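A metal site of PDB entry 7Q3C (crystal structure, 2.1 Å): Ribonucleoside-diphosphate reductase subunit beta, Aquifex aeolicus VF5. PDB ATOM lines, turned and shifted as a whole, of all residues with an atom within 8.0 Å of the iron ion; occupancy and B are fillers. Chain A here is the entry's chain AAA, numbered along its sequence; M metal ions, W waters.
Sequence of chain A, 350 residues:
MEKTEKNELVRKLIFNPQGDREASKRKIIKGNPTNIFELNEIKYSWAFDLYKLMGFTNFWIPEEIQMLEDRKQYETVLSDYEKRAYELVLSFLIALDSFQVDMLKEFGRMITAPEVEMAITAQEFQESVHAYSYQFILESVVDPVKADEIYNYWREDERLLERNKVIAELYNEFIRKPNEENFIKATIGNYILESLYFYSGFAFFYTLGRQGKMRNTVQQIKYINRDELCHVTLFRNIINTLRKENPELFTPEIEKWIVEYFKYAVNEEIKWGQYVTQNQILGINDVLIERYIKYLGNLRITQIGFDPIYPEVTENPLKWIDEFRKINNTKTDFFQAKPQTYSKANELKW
The iron ion is bound by water W1 (2.1 Å), water W2 (2.2 Å), OE1 of Glu 228 (2.2 Å), ND1 of His 231 (2.3 Å) and OE2 of Glu 127 (2.5 Å).
The iron ion has five donor atoms within binding distance.
Slightly farther from the iron ion lies OE2 of Glu 228 (2.7 Å).
Merely in contact with the iron ion: Glu 194 (3.9 Å).
Four residues have an atom within 4 Å of the iron ion: Glu 127, Glu 194, Glu 228 and His 231.
Along chain A the residues within 4 Å of the iron ion span positions 127 to 231.
The nearest printed residue that does not touch the iron ion is Gln 123 (4.2 Å).
Water W2 lies within hydrogen-bond range of the side-chain carboxylate (OE2) of Glu 194 (2.7 Å), the side-chain amide nitrogen (NE2) of Gln 123 (2.7 Å) and the side-chain amide nitrogen (NE2) of Gln 100 (2.8 Å).
The side-chain carboxylate (OE2) of Glu 228 sits close to a ring nitrogen (ND1) of His 130 (3.4 Å).
A ring nitrogen (NE2) of His 231 sits close to the backbone carbonyl oxygen of Asp 227 (3.3 Å).
The side-chain amide oxygen (OE1) of Gln 126 is in hydrogen-bond range of a ring nitrogen (NE2) of His 231, at 2.7 Å.
NE2 of His 231 lies close to SD of Met 54, at 3.8 Å.
The side-chain amide nitrogen (NE2) of Gln 123 lies within hydrogen-bond range of the side-chain carboxylate (OE2) of Glu 194, at 2.5 Å.
OE1 of Glu 194 lies within hydrogen-bond range of ND2 of Asn 190, at 2.8 Å.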
ATOM      1  N   MET A  54      24.756  32.424  34.931  1.00  0.00           N
ATOM      2  CA  MET A  54      25.698  31.276  34.878  1.00  0.00           C
ATOM      3  C   MET A  54      26.388  31.098  36.225  1.00  0.00           C
ATOM      4  O   MET A  54      26.627  29.944  36.626  1.00  0.00           O
ATOM      5  CB  MET A  54      26.767  31.492  33.802  1.00  0.00           C
ATOM      6  CG  MET A  54      26.260  31.298  32.400  1.00  0.00           C
ATOM      7  SD  MET A  54      27.632  31.177  31.231  1.00  0.00           S
ATOM      8  CE  MET A  54      27.915  32.916  30.917  1.00  0.00           C
ATOM      9  N   LEU A  96      34.919  17.363  24.565  1.00  0.00           N
ATOM     10  CA  LEU A  96      34.383  18.691  24.206  1.00  0.00           C
ATOM     11  C   LEU A  96      34.602  19.669  25.359  1.00  0.00           C
ATOM     12  O   LEU A  96      35.228  20.725  25.146  1.00  0.00           O
ATOM     13  CB  LEU A  96      32.877  18.596  23.911  1.00  0.00           C
ATOM     14  CG  LEU A  96      32.467  17.941  22.593  1.00  0.00           C
ATOM     15  CD1 LEU A  96      31.103  18.438  22.175  1.00  0.00           C
ATOM     16  CD2 LEU A  96      33.486  18.204  21.485  1.00  0.00           C
ATOM     17  N   ASP A  97      34.082  19.333  26.542  1.00  0.00           N
ATOM     18  CA  ASP A  97      34.112  20.224  27.728  1.00  0.00           C
ATOM     19  C   ASP A  97      35.580  20.483  28.104  1.00  0.00           C
ATOM     20  O   ASP A  97      35.862  21.618  28.515  1.00  0.00           O
ATOM     21  CB  ASP A  97      33.189  19.715  28.840  1.00  0.00           C
ATOM     22  CG  ASP A  97      31.718  20.082  28.643  1.00  0.00           C
ATOM     23  OD1 ASP A  97      31.454  21.187  28.146  1.00  0.00           O
ATOM     24  OD2 ASP A  97      30.841  19.257  28.965  1.00  0.00           O
ATOM     25  N   GLN A 100      36.870  23.085  25.810  1.00  0.00           N
ATOM     26  CA  GLN A 100      36.142  24.338  26.136  1.00  0.00           C
ATOM     27  C   GLN A 100      36.797  25.079  27.310  1.00  0.00           C
ATOM     28  O   GLN A 100      36.963  26.311  27.194  1.00  0.00           O
ATOM     29  CB  GLN A 100      34.674  24.040  26.411  1.00  0.00           C
ATOM     30  CG  GLN A 100      33.850  23.743  25.166  1.00  0.00           C
ATOM     31  CD  GLN A 100      34.037  24.782  24.094  1.00  0.00           C
ATOM     32  OE1 GLN A 100      34.847  24.627  23.181  1.00  0.00           O
ATOM     33  NE2 GLN A 100      33.323  25.887  24.228  1.00  0.00           N
ATOM     34  N   VAL A 101      37.132  24.376  28.397  1.00  0.00           N
ATOM     35  CA  VAL A 101      37.748  25.015  29.605  1.00  0.00           C
ATOM     36  C   VAL A 101      39.055  25.668  29.165  1.00  0.00           C
ATOM     37  O   VAL A 101      39.383  26.753  29.700  1.00  0.00           O
ATOM     38  CB  VAL A 101      37.986  24.030  30.771  1.00  0.00           C
ATOM     39  CG1 VAL A 101      36.681  23.639  31.443  1.00  0.00           C
ATOM     40  CG2 VAL A 101      38.737  22.787  30.367  1.00  0.00           C
ATOM     41  N   LEU A 104      38.442  28.706  26.250  1.00  0.00           N
ATOM     42  CA  LEU A 104      37.745  29.909  26.781  1.00  0.00           C
ATOM     43  C   LEU A 104      38.772  30.832  27.450  1.00  0.00           C
ATOM     44  O   LEU A 104      38.529  32.058  27.500  1.00  0.00           O
ATOM     45  CB  LEU A 104      36.608  29.488  27.721  1.00  0.00           C
ATOM     46  CG  LEU A 104      35.374  28.938  27.014  1.00  0.00           C
ATOM     47  CD1 LEU A 104      34.443  28.228  27.982  1.00  0.00           C
ATOM     48  CD2 LEU A 104      34.613  30.026  26.264  1.00  0.00           C
ATOM     49  N   GLN A 123      31.533  31.079  32.198  1.00  0.00           N
ATOM     50  CA  GLN A 123      31.417  29.965  31.232  1.00  0.00           C
ATOM     51  C   GLN A 123      32.533  28.947  31.467  1.00  0.00           C
ATOM     52  O   GLN A 123      32.239  27.748  31.514  1.00  0.00           O
ATOM     53  CB  GLN A 123      31.516  30.443  29.787  1.00  0.00           C
ATOM     54  CG  GLN A 123      31.201  29.315  28.809  1.00  0.00           C
ATOM     55  CD  GLN A 123      30.956  29.831  27.411  1.00  0.00           C
ATOM     56  OE1 GLN A 123      30.627  30.992  27.215  1.00  0.00           O
ATOM     57  NE2 GLN A 123      31.126  28.969  26.427  1.00  0.00           N
ATOM     58  N   GLU A 124      33.777  29.416  31.586  1.00  0.00           N
ATOM     59  CA  GLU A 124      34.960  28.555  31.781  1.00  0.00           C
ATOM     60  C   GLU A 124      34.749  27.715  33.047  1.00  0.00           C
ATOM     61  O   GLU A 124      35.080  26.515  33.027  1.00  0.00           O
ATOM     62  CB  GLU A 124      36.227  29.394  31.871  1.00  0.00           C
ATOM     63  CG  GLU A 124      37.496  28.567  31.944  1.00  0.00           C
ATOM     64  CD  GLU A 124      38.726  29.318  32.423  1.00  0.00           C
ATOM     65  OE1 GLU A 124      38.754  30.536  32.256  1.00  0.00           O
ATOM     66  OE2 GLU A 124      39.659  28.668  32.929  1.00  0.00           O
ATOM     67  N   GLN A 126      31.764  26.877  34.515  1.00  0.00           N
ATOM     68  CA  GLN A 126      30.681  25.901  34.213  1.00  0.00           C
ATOM     69  C   GLN A 126      31.268  24.710  33.453  1.00  0.00           C
ATOM     70  O   GLN A 126      30.919  23.561  33.788  1.00  0.00           O
ATOM     71  CB  GLN A 126      29.550  26.570  33.435  1.00  0.00           C
ATOM     72  CG  GLN A 126      28.744  27.523  34.290  1.00  0.00           C
ATOM     73  CD  GLN A 126      27.342  27.724  33.775  1.00  0.00           C
ATOM     74  OE1 GLN A 126      27.090  27.757  32.576  1.00  0.00           O
ATOM     75  NE2 GLN A 126      26.430  27.922  34.705  1.00  0.00           N
ATOM     76  N   GLU A 127      32.169  24.971  32.504  1.00  0.00           N
ATOM     77  CA  GLU A 127      32.864  23.899  31.737  1.00  0.00           C
ATOM     78  C   GLU A 127      33.660  23.016  32.705  1.00  0.00           C
ATOM     79  O   GLU A 127      33.681  21.791  32.490  1.00  0.00           O
ATOM     80  CB  GLU A 127      33.705  24.522  30.609  1.00  0.00           C
ATOM     81  CG  GLU A 127      32.869  25.212  29.540  1.00  0.00           C
ATOM     82  CD  GLU A 127      31.894  24.264  28.857  1.00  0.00           C
ATOM     83  OE1 GLU A 127      32.352  23.363  28.154  1.00  0.00           O
ATOM     84  OE2 GLU A 127      30.688  24.414  29.070  1.00  0.00           O
ATOM     85  N   HIS A 130      31.285  20.644  34.535  1.00  0.00           N
ATOM     86  CA  HIS A 130      30.897  19.538  33.621  1.00  0.00           C
ATOM     87  C   HIS A 130      31.961  18.444  33.700  1.00  0.00           C
ATOM     88  O   HIS A 130      31.574  17.275  33.823  1.00  0.00           O
ATOM     89  CB  HIS A 130      30.693  20.053  32.194  1.00  0.00           C
ATOM     90  CG  HIS A 130      29.611  21.077  32.106  1.00  0.00           C
ATOM     91  ND1 HIS A 130      29.293  21.703  30.918  1.00  0.00           N
ATOM     92  CD2 HIS A 130      28.810  21.605  33.051  1.00  0.00           C
ATOM     93  CE1 HIS A 130      28.319  22.571  31.137  1.00  0.00           C
ATOM     94  NE2 HIS A 130      28.026  22.542  32.448  1.00  0.00           N
ATOM     95  N   ASN A 190      33.314  27.764  18.126  1.00  0.00           N
ATOM     96  CA  ASN A 190      32.867  27.661  19.546  1.00  0.00           C
ATOM     97  C   ASN A 190      31.335  27.608  19.571  1.00  0.00           C
ATOM     98  O   ASN A 190      30.795  26.704  20.218  1.00  0.00           O
ATOM     99  CB  ASN A 190      33.439  28.791  20.392  1.00  0.00           C
ATOM    100  CG  ASN A 190      33.070  28.672  21.843  1.00  0.00           C
ATOM    101  OD1 ASN A 190      33.854  28.189  22.652  1.00  0.00           O
ATOM    102  ND2 ASN A 190      31.861  29.110  22.180  1.00  0.00           N
ATOM    103  N   LEU A 193      30.143  24.173  18.036  1.00  0.00           N
ATOM    104  CA  LEU A 193      30.407  23.148  19.079  1.00  0.00           C
ATOM    105  C   LEU A 193      29.312  23.201  20.150  1.00  0.00           C
ATOM    106  O   LEU A 193      28.858  22.122  20.561  1.00  0.00           O
ATOM    107  CB  LEU A 193      31.804  23.391  19.675  1.00  0.00           C
ATOM    108  CG  LEU A 193      32.244  22.439  20.785  1.00  0.00           C
ATOM    109  CD1 LEU A 193      33.756  22.345  20.847  1.00  0.00           C
ATOM    110  CD2 LEU A 193      31.677  22.841  22.142  1.00  0.00           C
ATOM    111  N   GLU A 194      28.920  24.397  20.589  1.00  0.00           N
ATOM    112  CA  GLU A 194      27.910  24.612  21.684  1.00  0.00           C
ATOM    113  C   GLU A 194      26.500  24.441  21.127  1.00  0.00           C
ATOM    114  O   GLU A 194      25.622  23.992  21.884  1.00  0.00           O
ATOM    115  CB  GLU A 194      28.017  26.017  22.269  1.00  0.00           C
ATOM    116  CG  GLU A 194      29.295  26.283  23.041  1.00  0.00           C
ATOM    117  CD  GLU A 194      29.555  27.748  23.328  1.00  0.00           C
ATOM    118  OE1 GLU A 194      29.092  28.620  22.537  1.00  0.00           O
ATOM    119  OE2 GLU A 194      30.220  28.038  24.327  1.00  0.00           O
ATOM    120  N   SER A 195      26.290  24.861  19.871  1.00  0.00           N
ATOM    121  CA  SER A 195      25.006  24.803  19.131  1.00  0.00           C
ATOM    122  C   SER A 195      24.573  23.354  18.882  1.00  0.00           C
ATOM    123  O   SER A 195      23.406  23.036  19.154  1.00  0.00           O
ATOM    124  CB  SER A 195      25.111  25.546  17.826  1.00  0.00           C
ATOM    125  OG  SER A 195      25.126  26.946  18.045  1.00  0.00           O
ATOM    126  N   PHE A 198      26.563  18.819  21.221  1.00  0.00           N
ATOM    127  CA  PHE A 198      26.064  18.263  22.504  1.00  0.00           C
ATOM    128  C   PHE A 198      24.772  17.462  22.299  1.00  0.00           C
ATOM    129  O   PHE A 198      24.428  16.650  23.184  1.00  0.00           O
ATOM    130  CB  PHE A 198      25.866  19.369  23.538  1.00  0.00           C
ATOM    131  CG  PHE A 198      27.143  19.813  24.220  1.00  0.00           C
ATOM    132  CD1 PHE A 198      27.627  19.121  25.326  1.00  0.00           C
ATOM    133  CD2 PHE A 198      27.860  20.903  23.762  1.00  0.00           C
ATOM    134  CE1 PHE A 198      28.799  19.516  25.940  1.00  0.00           C
ATOM    135  CE2 PHE A 198      29.042  21.289  24.374  1.00  0.00           C
ATOM    136  CZ  PHE A 198      29.507  20.598  25.468  1.00  0.00           C
ATOM    137  N   ILE A 224      23.790  20.239  32.782  1.00  0.00           N
ATOM    138  CA  ILE A 224      24.826  20.508  31.738  1.00  0.00           C
ATOM    139  C   ILE A 224      24.165  21.215  30.546  1.00  0.00           C
ATOM    140  O   ILE A 224      24.735  22.221  30.070  1.00  0.00           O
ATOM    141  CB  ILE A 224      25.550  19.208  31.307  1.00  0.00           C
ATOM    142  CG1 ILE A 224      26.450  18.684  32.421  1.00  0.00           C
ATOM    143  CG2 ILE A 224      26.329  19.427  30.012  1.00  0.00           C
ATOM    144  CD1 ILE A 224      26.956  17.285  32.194  1.00  0.00           C
ATOM    145  N   ASP A 227      23.221  24.818  31.051  1.00  0.00           N
ATOM    146  CA  ASP A 227      24.467  25.630  30.958  1.00  0.00           C
ATOM    147  C   ASP A 227      24.772  25.915  29.495  1.00  0.00           C
ATOM    148  O   ASP A 227      25.050  27.079  29.170  1.00  0.00           O
ATOM    149  CB  ASP A 227      25.653  24.914  31.644  1.00  0.00           C
ATOM    150  CG  ASP A 227      25.531  24.821  33.153  1.00  0.00           C
ATOM    151  OD1 ASP A 227      24.665  25.510  33.733  1.00  0.00           O
ATOM    152  OD2 ASP A 227      26.302  24.073  33.741  1.00  0.00           O
ATOM    153  N   GLU A 228      24.669  24.901  28.626  1.00  0.00           N
ATOM    154  CA  GLU A 228      25.008  24.997  27.179  1.00  0.00           C
ATOM    155  C   GLU A 228      24.107  26.001  26.454  1.00  0.00           C
ATOM    156  O   GLU A 228      24.590  26.613  25.483  1.00  0.00           O
ATOM    157  CB  GLU A 228      24.965  23.628  26.502  1.00  0.00           C
ATOM    158  CG  GLU A 228      26.098  22.719  26.920  1.00  0.00           C
ATOM    159  CD  GLU A 228      27.437  23.417  27.050  1.00  0.00           C
ATOM    160  OE1 GLU A 228      27.783  24.197  26.126  1.00  0.00           O
ATOM    161  OE2 GLU A 228      28.133  23.206  28.079  1.00  0.00           O
ATOM    162  N   LEU A 229      22.860  26.164  26.896  1.00  0.00           N
ATOM    163  CA  LEU A 229      21.913  27.155  26.300  1.00  0.00           C
ATOM    164  C   LEU A 229      22.426  28.570  26.575  1.00  0.00           C
ATOM    165  O   LEU A 229      22.411  29.390  25.645  1.00  0.00           O
ATOM    166  CB  LEU A 229      20.508  26.936  26.886  1.00  0.00           C
ATOM    167  CG  LEU A 229      19.876  25.579  26.569  1.00  0.00           C
ATOM    168  CD1 LEU A 229      18.505  25.460  27.213  1.00  0.00           C
ATOM    169  CD2 LEU A 229      19.775  25.342  25.070  1.00  0.00           C
ATOM    170  N   CYS A 230      22.869  28.857  27.801  1.00  0.00           N
ATOM    171  CA  CYS A 230      23.438  30.167  28.217  1.00  0.00           C
ATOM    172  C   CYS A 230      24.712  30.456  27.415  1.00  0.00           C
ATOM    173  O   CYS A 230      24.875  31.605  26.968  1.00  0.00           O
ATOM    174  CB  CYS A 230      23.765  30.189  29.702  1.00  0.00           C
ATOM    175  SG  CYS A 230      22.314  30.065  30.765  1.00  0.00           S
ATOM    176  N   HIS A 231      25.567  29.438  27.237  1.00  0.00           N
ATOM    177  CA  HIS A 231      26.834  29.514  26.464  1.00  0.00           C
ATOM    178  C   HIS A 231      26.536  29.866  25.012  1.00  0.00           C
ATOM    179  O   HIS A 231      27.169  30.813  24.493  1.00  0.00           O
ATOM    180  CB  HIS A 231      27.623  28.196  26.568  1.00  0.00           C
ATOM    181  CG  HIS A 231      27.945  27.796  27.967  1.00  0.00           C
ATOM    182  ND1 HIS A 231      28.728  26.709  28.264  1.00  0.00           N
ATOM    183  CD2 HIS A 231      27.603  28.355  29.146  1.00  0.00           C
ATOM    184  CE1 HIS A 231      28.828  26.583  29.568  1.00  0.00           C
ATOM    185  NE2 HIS A 231      28.135  27.582  30.130  1.00  0.00           N
ATOM    186  N   VAL A 232      25.603  29.154  24.380  1.00  0.00           N
ATOM    187  CA  VAL A 232      25.103  29.450  22.999  1.00  0.00           C
ATOM    188  C   VAL A 232      24.568  30.880  22.975  1.00  0.00           C
ATOM    189  O   VAL A 232      24.914  31.627  22.063  1.00  0.00           O
ATOM    190  CB  VAL A 232      24.039  28.422  22.540  1.00  0.00           C
ATOM    191  CG1 VAL A 232      23.224  28.897  21.345  1.00  0.00           C
ATOM    192  CG2 VAL A 232      24.678  27.077  22.239  1.00  0.00           C
ATOM    193  N   PHE A 235      27.595  33.444  23.068  1.00  0.00           N
ATOM    194  CA  PHE A 235      28.395  33.540  21.816  1.00  0.00           C
ATOM    195  C   PHE A 235      27.550  34.012  20.629  1.00  0.00           C
ATOM    196  O   PHE A 235      28.144  34.563  19.668  1.00  0.00           O
ATOM    197  CB  PHE A 235      29.131  32.221  21.546  1.00  0.00           C
ATOM    198  CG  PHE A 235      30.504  32.187  22.174  1.00  0.00           C
ATOM    199  CD1 PHE A 235      30.665  31.897  23.522  1.00  0.00           C
ATOM    200  CD2 PHE A 235      31.623  32.518  21.428  1.00  0.00           C
ATOM    201  CE1 PHE A 235      31.930  31.884  24.089  1.00  0.00           C
ATOM    202  CE2 PHE A 235      32.887  32.513  22.007  1.00  0.00           C
ATOM    203  CZ  PHE A 235      33.030  32.196  23.337  1.00  0.00           C
HETATM  204 FE    FE M   1      29.648  25.090  26.874  1.00  0.00          FE
HETATM  205  O   HOH W   1      30.657  23.383  26.136  1.00  0.00           O
HETATM  206  O   HOH W   2      31.241  26.275  26.043  1.00  0.00           O
